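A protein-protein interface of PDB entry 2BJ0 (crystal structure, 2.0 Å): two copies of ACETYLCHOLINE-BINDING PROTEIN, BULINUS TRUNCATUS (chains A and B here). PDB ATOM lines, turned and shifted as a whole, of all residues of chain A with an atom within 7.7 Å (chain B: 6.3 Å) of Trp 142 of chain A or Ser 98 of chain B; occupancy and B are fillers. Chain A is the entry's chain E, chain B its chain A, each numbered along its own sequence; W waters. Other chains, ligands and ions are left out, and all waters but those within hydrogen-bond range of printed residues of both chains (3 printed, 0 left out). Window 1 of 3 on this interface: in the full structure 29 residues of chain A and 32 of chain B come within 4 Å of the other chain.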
ATOM      1  N   PRO A  83       5.662 -12.740 -38.530  1.00  0.00           N
ATOM      2  CA  PRO A  83       5.459 -12.828 -37.072  1.00  0.00           C
ATOM      3  C   PRO A  83       5.689 -11.514 -36.350  1.00  0.00           C
ATOM      4  O   PRO A  83       6.673 -10.831 -36.618  1.00  0.00           O
ATOM      5  CB  PRO A  83       6.541 -13.828 -36.626  1.00  0.00           C
ATOM      6  CG  PRO A  83       6.879 -14.589 -37.867  1.00  0.00           C
ATOM      7  CD  PRO A  83       6.784 -13.583 -38.969  1.00  0.00           C
ATOM      8  N   ASP A  84       4.820 -11.195 -35.382  1.00  0.00           N
ATOM      9  CA  ASP A  84       4.995  -9.968 -34.631  1.00  0.00           C
ATOM     10  C   ASP A  84       5.906 -10.161 -33.418  1.00  0.00           C
ATOM     11  O   ASP A  84       5.511  -9.951 -32.255  1.00  0.00           O
ATOM     12  CB  ASP A  84       3.634  -9.415 -34.232  1.00  0.00           C
ATOM     13  CG  ASP A  84       2.946 -10.294 -33.230  1.00  0.00           C
ATOM     14  OD1 ASP A  84       3.116 -11.549 -33.308  1.00  0.00           O
ATOM     15  OD2 ASP A  84       2.248  -9.814 -32.310  1.00  0.00           O
ATOM     16  N   LEU A  85       7.141 -10.552 -33.692  1.00  0.00           N
ATOM     17  CA  LEU A  85       8.124 -10.822 -32.644  1.00  0.00           C
ATOM     18  C   LEU A  85       8.466  -9.541 -31.923  1.00  0.00           C
ATOM     19  O   LEU A  85       8.577  -8.494 -32.538  1.00  0.00           O
ATOM     20  CB  LEU A  85       9.410 -11.422 -33.251  1.00  0.00           C
ATOM     21  CG  LEU A  85       9.174 -12.791 -33.891  1.00  0.00           C
ATOM     22  CD1 LEU A  85      10.470 -13.289 -34.582  1.00  0.00           C
ATOM     23  CD2 LEU A  85       8.625 -13.837 -32.919  1.00  0.00           C
ATOM     24  N   SER A  86       8.612  -9.602 -30.611  1.00  0.00           N
ATOM     25  CA  SER A  86       9.072  -8.449 -29.889  1.00  0.00           C
ATOM     26  C   SER A  86      10.071  -8.899 -28.866  1.00  0.00           C
ATOM     27  O   SER A  86      10.052 -10.056 -28.488  1.00  0.00           O
ATOM     28  CB  SER A  86       7.900  -7.760 -29.207  1.00  0.00           C
ATOM     29  OG  SER A  86       7.028  -7.249 -30.187  1.00  0.00           O
ATOM     30  N   PHE A  87      10.950  -7.993 -28.448  1.00  0.00           N
ATOM     31  CA  PHE A  87      11.833  -8.243 -27.338  1.00  0.00           C
ATOM     32  C   PHE A  87      11.120  -7.772 -26.075  1.00  0.00           C
ATOM     33  O   PHE A  87      10.908  -6.572 -25.871  1.00  0.00           O
ATOM     34  CB  PHE A  87      13.129  -7.510 -27.552  1.00  0.00           C
ATOM     35  CG  PHE A  87      13.866  -7.972 -28.777  1.00  0.00           C
ATOM     36  CD1 PHE A  87      14.675  -9.093 -28.724  1.00  0.00           C
ATOM     37  CD2 PHE A  87      13.742  -7.294 -29.977  1.00  0.00           C
ATOM     38  CE1 PHE A  87      15.349  -9.540 -29.828  1.00  0.00           C
ATOM     39  CE2 PHE A  87      14.426  -7.732 -31.108  1.00  0.00           C
ATOM     40  CZ  PHE A  87      15.221  -8.867 -31.036  1.00  0.00           C
ATOM     41  N   TYR A  88      10.720  -8.714 -25.233  1.00  0.00           N
ATOM     42  CA  TYR A  88       9.933  -8.364 -24.039  1.00  0.00           C
ATOM     43  C   TYR A  88      10.700  -7.439 -23.140  1.00  0.00           C
ATOM     44  O   TYR A  88      10.106  -6.613 -22.448  1.00  0.00           O
ATOM     45  CB  TYR A  88       9.542  -9.605 -23.248  1.00  0.00           C
ATOM     46  CG  TYR A  88       8.283 -10.230 -23.738  1.00  0.00           C
ATOM     47  CD1 TYR A  88       8.239 -10.848 -24.983  1.00  0.00           C
ATOM     48  CD2 TYR A  88       7.124 -10.213 -22.960  1.00  0.00           C
ATOM     49  CE1 TYR A  88       7.081 -11.434 -25.445  1.00  0.00           C
ATOM     50  CE2 TYR A  88       5.949 -10.791 -23.417  1.00  0.00           C
ATOM     51  CZ  TYR A  88       5.935 -11.413 -24.657  1.00  0.00           C
ATOM     52  OH  TYR A  88       4.781 -11.988 -25.149  1.00  0.00           O
ATOM     53  N   ASN A  89      12.023  -7.576 -23.157  1.00  0.00           N
ATOM     54  CA  ASN A  89      12.874  -6.763 -22.301  1.00  0.00           C
ATOM     55  C   ASN A  89      13.663  -5.662 -23.009  1.00  0.00           C
ATOM     56  O   ASN A  89      14.617  -5.136 -22.450  1.00  0.00           O
ATOM     57  CB  ASN A  89      13.797  -7.631 -21.400  1.00  0.00           C
ATOM     58  CG  ASN A  89      14.811  -8.452 -22.182  1.00  0.00           C
ATOM     59  OD1 ASN A  89      14.502  -9.015 -23.243  1.00  0.00           O
ATOM     60  ND2 ASN A  89      16.020  -8.569 -21.634  1.00  0.00           N
ATOM     61  N   ALA A  90      13.262  -5.291 -24.223  1.00  0.00           N
ATOM     62  CA  ALA A  90      13.875  -4.127 -24.880  1.00  0.00           C
ATOM     63  C   ALA A  90      13.553  -2.820 -24.109  1.00  0.00           C
ATOM     64  O   ALA A  90      12.440  -2.634 -23.570  1.00  0.00           O
ATOM     65  CB  ALA A  90      13.424  -4.041 -26.333  1.00  0.00           C
ATOM     66  N   ALA A  92      14.818   0.075 -25.768  1.00  0.00           N
ATOM     67  CA  ALA A  92      14.796   1.012 -26.900  1.00  0.00           C
ATOM     68  C   ALA A  92      14.232   0.229 -28.061  1.00  0.00           C
ATOM     69  O   ALA A  92      14.268  -0.990 -28.033  1.00  0.00           O
ATOM     70  CB  ALA A  92      16.197   1.530 -27.214  1.00  0.00           C
ATOM     71  N   ALA A  93      13.644   0.900 -29.038  1.00  0.00           N
ATOM     72  CA  ALA A  93      13.038   0.196 -30.149  1.00  0.00           C
ATOM     73  C   ALA A  93      14.188  -0.478 -30.942  1.00  0.00           C
ATOM     74  O   ALA A  93      15.227   0.128 -31.139  1.00  0.00           O
ATOM     75  CB  ALA A  93      12.248   1.158 -31.034  1.00  0.00           C
ATOM     76  N   PRO A  94      14.049  -1.740 -31.309  1.00  0.00           N
ATOM     77  CA  PRO A  94      15.105  -2.415 -32.059  1.00  0.00           C
ATOM     78  C   PRO A  94      15.330  -1.769 -33.436  1.00  0.00           C
ATOM     79  O   PRO A  94      14.379  -1.343 -34.064  1.00  0.00           O
ATOM     80  CB  PRO A  94      14.575  -3.825 -32.209  1.00  0.00           C
ATOM     81  CG  PRO A  94      13.540  -3.927 -31.123  1.00  0.00           C
ATOM     82  CD  PRO A  94      12.910  -2.617 -31.023  1.00  0.00           C
ATOM     83  N   VAL A 139      12.305 -13.170 -26.248  1.00  0.00           N
ATOM     84  CA  VAL A 139      11.690 -12.942 -27.567  1.00  0.00           C
ATOM     85  C   VAL A 139      10.459 -13.786 -27.770  1.00  0.00           C
ATOM     86  O   VAL A 139      10.493 -14.989 -27.552  1.00  0.00           O
ATOM     87  CB  VAL A 139      12.667 -13.334 -28.736  1.00  0.00           C
ATOM     88  CG1 VAL A 139      12.034 -13.079 -30.088  1.00  0.00           C
ATOM     89  CG2 VAL A 139      13.965 -12.576 -28.634  1.00  0.00           C
ATOM     90  N   GLY A 140       9.401 -13.180 -28.284  1.00  0.00           N
ATOM     91  CA  GLY A 140       8.147 -13.901 -28.483  1.00  0.00           C
ATOM     92  C   GLY A 140       7.136 -13.039 -29.211  1.00  0.00           C
ATOM     93  O   GLY A 140       7.390 -11.859 -29.451  1.00  0.00           O
ATOM     94  N   SER A 141       6.011 -13.629 -29.613  1.00  0.00           N
ATOM     95  CA  SER A 141       4.973 -12.850 -30.274  1.00  0.00           C
ATOM     96  C   SER A 141       4.347 -11.933 -29.240  1.00  0.00           C
ATOM     97  O   SER A 141       4.053 -12.382 -28.128  1.00  0.00           O
ATOM     98  CB  SER A 141       3.898 -13.780 -30.799  1.00  0.00           C
ATOM     99  OG  SER A 141       2.746 -13.045 -31.134  1.00  0.00           O
ATOM    100  N   TRP A 142       4.117 -10.675 -29.602  1.00  0.00           N
ATOM    101  CA  TRP A 142       3.457  -9.748 -28.694  1.00  0.00           C
ATOM    102  C   TRP A 142       1.970  -9.996 -28.531  1.00  0.00           C
ATOM    103  O   TRP A 142       1.407  -9.722 -27.463  1.00  0.00           O
ATOM    104  CB  TRP A 142       3.681  -8.305 -29.162  1.00  0.00           C
ATOM    105  CG  TRP A 142       3.407  -7.255 -28.106  1.00  0.00           C
ATOM    106  CD1 TRP A 142       2.419  -6.326 -28.121  1.00  0.00           C
ATOM    107  CD2 TRP A 142       4.141  -7.039 -26.902  1.00  0.00           C
ATOM    108  NE1 TRP A 142       2.494  -5.538 -27.003  1.00  0.00           N
ATOM    109  CE2 TRP A 142       3.539  -5.966 -26.228  1.00  0.00           C
ATOM    110  CE3 TRP A 142       5.244  -7.652 -26.314  1.00  0.00           C
ATOM    111  CZ2 TRP A 142       4.007  -5.494 -25.009  1.00  0.00           C
ATOM    112  CZ3 TRP A 142       5.718  -7.168 -25.101  1.00  0.00           C
ATOM    113  CH2 TRP A 142       5.111  -6.094 -24.479  1.00  0.00           C
ATOM    114  N   THR A 143       1.306 -10.456 -29.586  1.00  0.00           N
ATOM    115  CA  THR A 143      -0.146 -10.536 -29.586  1.00  0.00           C
ATOM    116  C   THR A 143      -0.720 -11.855 -30.058  1.00  0.00           C
ATOM    117  O   THR A 143      -1.942 -11.965 -30.158  1.00  0.00           O
ATOM    118  CB  THR A 143      -0.756  -9.428 -30.427  1.00  0.00           C
ATOM    119  OG1 THR A 143      -0.267  -9.515 -31.788  1.00  0.00           O
ATOM    120  CG2 THR A 143      -0.336  -8.040 -29.887  1.00  0.00           C
ATOM    121  N   HIS A 144       0.112 -12.848 -30.373  1.00  0.00           N
ATOM    122  CA  HIS A 144      -0.428 -14.167 -30.774  1.00  0.00           C
ATOM    123  C   HIS A 144      -0.128 -15.193 -29.688  1.00  0.00           C
ATOM    124  O   HIS A 144       1.007 -15.588 -29.519  1.00  0.00           O
ATOM    125  CB  HIS A 144       0.125 -14.635 -32.146  1.00  0.00           C
ATOM    126  CG  HIS A 144      -0.281 -13.754 -33.288  1.00  0.00           C
ATOM    127  ND1 HIS A 144       0.521 -12.745 -33.785  1.00  0.00           N
ATOM    128  CD2 HIS A 144      -1.420 -13.723 -34.019  1.00  0.00           C
ATOM    129  CE1 HIS A 144      -0.113 -12.126 -34.767  1.00  0.00           C
ATOM    130  NE2 HIS A 144      -1.290 -12.709 -34.934  1.00  0.00           N
ATOM    131  N   ASP A 145      -1.145 -15.599 -28.929  1.00  0.00           N
ATOM    132  CA  ASP A 145      -0.933 -16.559 -27.842  1.00  0.00           C
ATOM    133  C   ASP A 145      -0.667 -17.916 -28.408  1.00  0.00           C
ATOM    134  O   ASP A 145      -0.732 -18.096 -29.619  1.00  0.00           O
ATOM    135  CB  ASP A 145      -2.090 -16.574 -26.842  1.00  0.00           C
ATOM    136  CG  ASP A 145      -3.395 -17.038 -27.445  1.00  0.00           C
ATOM    137  OD1 ASP A 145      -3.418 -17.862 -28.371  1.00  0.00           O
ATOM    138  OD2 ASP A 145      -4.484 -16.628 -27.021  1.00  0.00           O
ATOM    139  N   PHE A 149       0.005 -19.433 -32.250  1.00  0.00           N
ATOM    140  CA  PHE A 149       1.380 -19.185 -32.651  1.00  0.00           C
ATOM    141  C   PHE A 149       2.266 -20.021 -31.753  1.00  0.00           C
ATOM    142  O   PHE A 149       2.479 -19.703 -30.593  1.00  0.00           O
ATOM    143  CB  PHE A 149       1.640 -17.675 -32.490  1.00  0.00           C
ATOM    144  CG  PHE A 149       3.011 -17.193 -32.919  1.00  0.00           C
ATOM    145  CD1 PHE A 149       4.145 -17.465 -32.147  1.00  0.00           C
ATOM    146  CD2 PHE A 149       3.140 -16.341 -34.016  1.00  0.00           C
ATOM    147  CE1 PHE A 149       5.408 -16.974 -32.497  1.00  0.00           C
ATOM    148  CE2 PHE A 149       4.403 -15.830 -34.372  1.00  0.00           C
ATOM    149  CZ  PHE A 149       5.538 -16.147 -33.601  1.00  0.00           C
ATOM    150  N   TYR A 184       0.299 -13.740 -18.791  1.00  0.00           N
ATOM    151  CA  TYR A 184       0.431 -12.337 -18.354  1.00  0.00           C
ATOM    152  C   TYR A 184      -0.863 -11.788 -17.760  1.00  0.00           C
ATOM    153  O   TYR A 184      -1.966 -12.184 -18.167  1.00  0.00           O
ATOM    154  CB  TYR A 184       0.937 -11.440 -19.492  1.00  0.00           C
ATOM    155  CG  TYR A 184       2.293 -11.871 -19.953  1.00  0.00           C
ATOM    156  CD1 TYR A 184       3.435 -11.431 -19.303  1.00  0.00           C
ATOM    157  CD2 TYR A 184       2.429 -12.775 -20.999  1.00  0.00           C
ATOM    158  CE1 TYR A 184       4.672 -11.851 -19.698  1.00  0.00           C
ATOM    159  CE2 TYR A 184       3.677 -13.207 -21.414  1.00  0.00           C
ATOM    160  CZ  TYR A 184       4.793 -12.743 -20.759  1.00  0.00           C
ATOM    161  OH  TYR A 184       6.040 -13.163 -21.149  1.00  0.00           O
ATOM    162  N   CYS A 186      -2.485  -9.065 -17.931  1.00  0.00           N
ATOM    163  CA  CYS A 186      -3.433  -8.348 -18.786  1.00  0.00           C
ATOM    164  C   CYS A 186      -4.361  -9.293 -19.548  1.00  0.00           C
ATOM    165  O   CYS A 186      -5.429  -8.895 -20.020  1.00  0.00           O
ATOM    166  CB  CYS A 186      -2.662  -7.498 -19.797  1.00  0.00           C
ATOM    167  SG  CYS A 186      -1.545  -8.484 -20.825  1.00  0.00           S
ATOM    168  N   CYS A 187      -3.947 -10.551 -19.655  1.00  0.00           N
ATOM    169  CA  CYS A 187      -4.358 -11.355 -20.783  1.00  0.00           C
ATOM    170  C   CYS A 187      -4.656 -12.806 -20.409  1.00  0.00           C
ATOM    171  O   CYS A 187      -4.043 -13.365 -19.498  1.00  0.00           O
ATOM    172  CB  CYS A 187      -3.265 -11.235 -21.856  1.00  0.00           C
ATOM    173  SG  CYS A 187      -2.768  -9.491 -22.171  1.00  0.00           S
ATOM    174  N   TYR A 191       1.663 -17.263 -23.614  1.00  0.00           N
ATOM    175  CA  TYR A 191       2.509 -16.912 -24.743  1.00  0.00           C
ATOM    176  C   TYR A 191       3.802 -17.669 -24.630  1.00  0.00           C
ATOM    177  O   TYR A 191       4.405 -17.709 -23.557  1.00  0.00           O
ATOM    178  CB  TYR A 191       2.784 -15.405 -24.739  1.00  0.00           C
ATOM    179  CG  TYR A 191       1.565 -14.610 -25.103  1.00  0.00           C
ATOM    180  CD1 TYR A 191       0.516 -14.461 -24.198  1.00  0.00           C
ATOM    181  CD2 TYR A 191       1.436 -14.038 -26.365  1.00  0.00           C
ATOM    182  CE1 TYR A 191      -0.617 -13.762 -24.532  1.00  0.00           C
ATOM    183  CE2 TYR A 191       0.293 -13.322 -26.708  1.00  0.00           C
ATOM    184  CZ  TYR A 191      -0.723 -13.194 -25.781  1.00  0.00           C
ATOM    185  OH  TYR A 191      -1.872 -12.505 -26.099  1.00  0.00           O
ATOM    186  N   ASP A 192       4.220 -18.270 -25.740  1.00  0.00           N
ATOM    187  CA  ASP A 192       5.545 -18.863 -25.879  1.00  0.00           C
ATOM    188  C   ASP A 192       6.562 -17.749 -25.925  1.00  0.00           C
ATOM    189  O   ASP A 192       6.288 -16.687 -26.471  1.00  0.00           O
ATOM    190  CB  ASP A 192       5.651 -19.641 -27.202  1.00  0.00           C
ATOM    191  CG  ASP A 192       4.926 -20.978 -27.178  1.00  0.00           C
ATOM    192  OD1 ASP A 192       4.477 -21.418 -26.086  1.00  0.00           O
ATOM    193  OD2 ASP A 192       4.761 -21.659 -28.218  1.00  0.00           O
ATOM    194  N   TRP B  51       4.335  -0.413 -19.852  1.00  0.00           N
ATOM    195  CA  TRP B  51       3.241  -0.955 -20.655  1.00  0.00           C
ATOM    196  C   TRP B  51       1.959  -0.270 -20.249  1.00  0.00           C
ATOM    197  O   TRP B  51       1.699  -0.141 -19.056  1.00  0.00           O
ATOM    198  CB  TRP B  51       3.060  -2.448 -20.409  1.00  0.00           C
ATOM    199  CG  TRP B  51       4.241  -3.304 -20.672  1.00  0.00           C
ATOM    200  CD1 TRP B  51       5.477  -2.926 -21.189  1.00  0.00           C
ATOM    201  CD2 TRP B  51       4.314  -4.716 -20.464  1.00  0.00           C
ATOM    202  NE1 TRP B  51       6.287  -4.035 -21.314  1.00  0.00           N
ATOM    203  CE2 TRP B  51       5.605  -5.142 -20.881  1.00  0.00           C
ATOM    204  CE3 TRP B  51       3.417  -5.679 -19.963  1.00  0.00           C
ATOM    205  CZ2 TRP B  51       6.016  -6.470 -20.795  1.00  0.00           C
ATOM    206  CZ3 TRP B  51       3.836  -7.016 -19.892  1.00  0.00           C
ATOM    207  CH2 TRP B  51       5.116  -7.388 -20.312  1.00  0.00           C
ATOM    208  N   GLU B  95       8.707   6.300 -27.187  1.00  0.00           N
ATOM    209  CA  GLU B  95       9.213   5.411 -28.205  1.00  0.00           C
ATOM    210  C   GLU B  95       8.543   4.077 -28.017  1.00  0.00           C
ATOM    211  O   GLU B  95       8.571   3.500 -26.912  1.00  0.00           O
ATOM    212  CB  GLU B  95      10.728   5.273 -28.085  1.00  0.00           C
ATOM    213  CG  GLU B  95      11.328   4.419 -29.191  1.00  0.00           C
ATOM    214  CD  GLU B  95      12.834   4.479 -29.212  1.00  0.00           C
ATOM    215  OE1 GLU B  95      13.468   3.833 -28.371  1.00  0.00           O
ATOM    216  OE2 GLU B  95      13.391   5.193 -30.083  1.00  0.00           O
ATOM    217  N   LEU B  96       7.885   3.610 -29.075  1.00  0.00           N
ATOM    218  CA  LEU B  96       7.240   2.318 -29.050  1.00  0.00           C
ATOM    219  C   LEU B  96       8.257   1.191 -29.153  1.00  0.00           C
ATOM    220  O   LEU B  96       9.141   1.188 -30.054  1.00  0.00           O
ATOM    221  CB  LEU B  96       6.189   2.229 -30.157  1.00  0.00           C
ATOM    222  CG  LEU B  96       5.424   0.924 -30.319  1.00  0.00           C
ATOM    223  CD1 LEU B  96       4.444   0.768 -29.169  1.00  0.00           C
ATOM    224  CD2 LEU B  96       4.687   0.949 -31.679  1.00  0.00           C
ATOM    225  N   LEU B  97       8.129   0.226 -28.235  1.00  0.00           N
ATOM    226  CA  LEU B  97       9.096  -0.860 -28.087  1.00  0.00           C
ATOM    227  C   LEU B  97       8.565  -2.250 -28.456  1.00  0.00           C
ATOM    228  O   LEU B  97       9.296  -3.252 -28.404  1.00  0.00           O
ATOM    229  CB  LEU B  97       9.615  -0.866 -26.641  1.00  0.00           C
ATOM    230  CG  LEU B  97      10.102   0.433 -25.992  1.00  0.00           C
ATOM    231  CD1 LEU B  97      10.368   0.208 -24.482  1.00  0.00           C
ATOM    232  CD2 LEU B  97      11.377   0.873 -26.669  1.00  0.00           C
ATOM    233  N   SER B  98       7.302  -2.336 -28.830  1.00  0.00           N
ATOM    234  CA  SER B  98       6.659  -3.633 -29.074  1.00  0.00           C
ATOM    235  C   SER B  98       5.917  -3.522 -30.415  1.00  0.00           C
ATOM    236  O   SER B  98       5.769  -2.424 -30.939  1.00  0.00           O
ATOM    237  CB  SER B  98       5.639  -3.889 -27.967  1.00  0.00           C
ATOM    238  OG  SER B  98       4.777  -2.768 -27.865  1.00  0.00           O
ATOM    239  N   ALA B  99       5.428  -4.644 -30.943  1.00  0.00           N
ATOM    240  CA  ALA B  99       4.676  -4.672 -32.201  1.00  0.00           C
ATOM    241  C   ALA B  99       3.357  -3.912 -32.054  1.00  0.00           C
ATOM    242  O   ALA B  99       2.688  -4.022 -31.036  1.00  0.00           O
ATOM    243  CB  ALA B  99       4.401  -6.101 -32.596  1.00  0.00           C
ATOM    244  N   ASP B 100       2.983  -3.136 -33.066  1.00  0.00           N
ATOM    245  CA  ASP B 100       1.808  -2.264 -32.945  1.00  0.00           C
ATOM    246  C   ASP B 100       0.542  -2.938 -33.461  1.00  0.00           C
ATOM    247  O   ASP B 100       0.110  -2.704 -34.593  1.00  0.00           O
ATOM    248  CB  ASP B 100       2.059  -0.940 -33.668  1.00  0.00           C
ATOM    249  CG  ASP B 100       1.415   0.236 -32.974  1.00  0.00           C
ATOM    250  OD1 ASP B 100       0.908   0.071 -31.833  1.00  0.00           O
ATOM    251  OD2 ASP B 100       1.373   1.370 -33.495  1.00  0.00           O
ATOM    252  N   ARG B 101      -0.056  -3.770 -32.606  1.00  0.00           N
ATOM    253  CA  ARG B 101      -1.189  -4.573 -32.965  1.00  0.00           C
ATOM    254  C   ARG B 101      -2.191  -4.604 -31.816  1.00  0.00           C
ATOM    255  O   ARG B 101      -1.800  -4.488 -30.673  1.00  0.00           O
ATOM    256  CB  ARG B 101      -0.752  -5.993 -33.209  1.00  0.00           C
ATOM    257  CG  ARG B 101       0.035  -6.219 -34.459  1.00  0.00           C
ATOM    258  CD  ARG B 101       0.084  -7.678 -34.819  1.00  0.00           C
ATOM    259  NE  ARG B 101       0.110  -7.825 -36.264  1.00  0.00           N
ATOM    260  CZ  ARG B 101      -0.794  -8.441 -37.000  1.00  0.00           C
ATOM    261  NH1 ARG B 101      -1.846  -9.025 -36.478  1.00  0.00           N
ATOM    262  NH2 ARG B 101      -0.616  -8.492 -38.300  1.00  0.00           N
ATOM    263  N   VAL B 103      -5.784  -6.828 -30.245  1.00  0.00           N
ATOM    264  CA  VAL B 103      -6.444  -8.126 -30.264  1.00  0.00           C
ATOM    265  C   VAL B 103      -7.914  -7.941 -29.983  1.00  0.00           C
ATOM    266  O   VAL B 103      -8.290  -7.358 -28.965  1.00  0.00           O
ATOM    267  CB  VAL B 103      -5.878  -9.088 -29.222  1.00  0.00           C
ATOM    268  CG1 VAL B 103      -6.703 -10.388 -29.205  1.00  0.00           C
ATOM    269  CG2 VAL B 103      -4.376  -9.366 -29.476  1.00  0.00           C
ATOM    270  N   VAL B 113      -1.827  -3.113 -25.913  1.00  0.00           N
ATOM    271  CA  VAL B 113      -0.813  -3.031 -24.879  1.00  0.00           C
ATOM    272  C   VAL B 113       0.483  -2.590 -25.508  1.00  0.00           C
ATOM    273  O   VAL B 113       1.331  -3.411 -25.768  1.00  0.00           O
ATOM    274  CB  VAL B 113      -0.587  -4.381 -24.142  1.00  0.00           C
ATOM    275  CG1 VAL B 113       0.390  -4.188 -22.942  1.00  0.00           C
ATOM    276  CG2 VAL B 113      -1.903  -4.968 -23.644  1.00  0.00           C
ATOM    277  N   PRO B 114       0.641  -1.295 -25.734  1.00  0.00           N
ATOM    278  CA  PRO B 114       1.923  -0.776 -26.178  1.00  0.00           C
ATOM    279  C   PRO B 114       3.004  -0.760 -25.056  1.00  0.00           C
ATOM    280  O   PRO B 114       2.719  -0.317 -23.949  1.00  0.00           O
ATOM    281  CB  PRO B 114       1.591   0.666 -26.629  1.00  0.00           C
ATOM    282  CG  PRO B 114       0.317   1.048 -25.953  1.00  0.00           C
ATOM    283  CD  PRO B 114      -0.386  -0.238 -25.586  1.00  0.00           C
ATOM    284  N   SER B 115       4.216  -1.248 -25.332  1.00  0.00           N
ATOM    285  CA  SER B 115       5.326  -0.957 -24.438  1.00  0.00           C
ATOM    286  C   SER B 115       6.046   0.300 -24.932  1.00  0.00           C
ATOM    287  O   SER B 115       6.511   0.316 -26.115  1.00  0.00           O
ATOM    288  CB  SER B 115       6.281  -2.143 -24.362  1.00  0.00           C
ATOM    289  OG  SER B 115       7.353  -1.840 -23.457  1.00  0.00           O
ATOM    290  N   GLN B 116       6.169   1.339 -24.089  1.00  0.00           N
ATOM    291  CA  GLN B 116       6.853   2.589 -24.526  1.00  0.00           C
ATOM    292  C   GLN B 116       7.881   3.093 -23.539  1.00  0.00           C
ATOM    293  O   GLN B 116       7.705   2.976 -22.312  1.00  0.00           O
ATOM    294  CB  GLN B 116       5.863   3.729 -24.797  1.00  0.00           C
ATOM    295  CG  GLN B 116       4.687   3.369 -25.745  1.00  0.00           C
ATOM    296  CD  GLN B 116       3.544   4.335 -25.610  1.00  0.00           C
ATOM    297  OE1 GLN B 116       2.739   4.269 -24.640  1.00  0.00           O
ATOM    298  NE2 GLN B 116       3.456   5.243 -26.533  1.00  0.00           N
HETATM  299  O   HOH W   1       9.074  -4.693 -26.066  1.00  0.00           O
HETATM  300  O   HOH W   2      10.749  -5.349 -29.551  1.00  0.00           O
HETATM  301  O   HOH W   3       9.483  -3.317 -23.917  1.00  0.00           O
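Gly 140 of chain A touches none of the printed residues of chain B.
Trp 142 of chain A touches just these residues of chain B: Trp 51 (3.8 Å), Ser 98 (3.4 Å), Ala 99 (3.7 Å) and Val 113 (2.7 Å).
Of the printed residues of chain A, Glu 95 of chain B touches Ala 92 and Ala 93.
Of chain A, only Ser 86 and Trp 142 come within 4 Å of Ser 98 of chain B.
Asp 100 of chain B touches none of the printed residues of chain A.
Printed residues of chain A within 4 Å of Val 113 of chain B: Trp 142 (2.7 Å).
The nearest printed residue of chain A that does not touch Ser 98 of chain B is Leu 85 of chain A (6.0 Å).
CD of Arg 101 of chain B touches OD2 of Asp 84 of chain A (3.9 Å).
Ala 90 of chain A touches Leu 97 of chain B.
OE1 of Glu 95 of chain B touches CA of Ala 92 of chain A, 3.4 Å away.
Leu 96 of chain B touches Ala 93 of chain A.
Ala 93 of chain A touches Leu 97 of chain B.
Trp 51 of chain B touches Trp 142 of chain A (CE2 to CH2, 3.8 Å).
Ser 98 of chain B touches Trp 142 of chain A (CB to CE2, 3.4 Å).
Ala 99 of chain B touches Trp 142 of chain A (O to CD1, 3.7 Å).
CD of Arg 101 of chain B touches OG1 of Thr 143 of chain A, 3.6 Å away.
O of Thr 143 of chain A touches CG2 of Val 103 of chain B, 3.6 Å away.
NE1 of Trp 51 of chain B sits close to OG of Ser 115 of chain B (3.2 Å).
N of Leu 97 of chain B sits at hydrogen-bond distance from O of Ser 115 of chain B (2.7 Å).
The side-chain carboxylate (OD1) of Asp 84 of chain A sits at hydrogen-bond distance from the side-chain hydroxyl (OG) of Ser 141 of chain A, at 2.7 Å.
The side-chain hydroxyl (OG1) of Thr 143 of chain A is in hydrogen-bond range of the side-chain carboxylate (OD2) of Asp 84 of chain A.
N of Thr 143 of chain A is in hydrogen-bond range of OG of Ser 141 of chain A (3.3 Å).
The side-chain sulfur (SG) of Cys 186 of chain A is disulfide-bonded to the side-chain sulfur (SG) of Cys 187 of chain A, 2.1 Å away.
Water W3 lies within hydrogen-bond range of the side-chain hydroxyl (OG) of Ser 115 of chain B (2.6 Å) and the backbone carbonyl oxygen (O) of Ala 90 of chain A (3.1 Å).
Water W1 bridges O of Phe 87 of chain A and O of Leu 97 of chain B.
Water W2 lies within hydrogen-bond range of O of Leu 97 of chain B and N of Phe 87 of chain A.
No position is printed for both chains.
Of the 17 pairs that touch across the chains among the printed residues, none has its exchanged pair printed and touching as well.
Hydrophobic or aromatic side chains of chain B within 4 Å of the printed part of chain A: Trp 51, Leu 97, Ala 99 and Val 103.
Along chain B the printed residues that touch a printed residue of chain A span positions 51 to 113.
Among the printed residues, no Asp or Glu carboxylate lies within 4 Å of a Lys or Arg side-chain nitrogen of the other chain.
N of Ala 93 of chain A sits at hydrogen-bond distance from OE1 of Glu 95 of chain B, at 3.0 Å.
N of Ala 99 of chain B lies within hydrogen-bond range of OG of Ser 86 of chain A.
The indole nitrogen of Trp 142 of chain A lies within hydrogen-bond range of the backbone carbonyl oxygen of Val 113 of chain B, at 2.7 Å.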
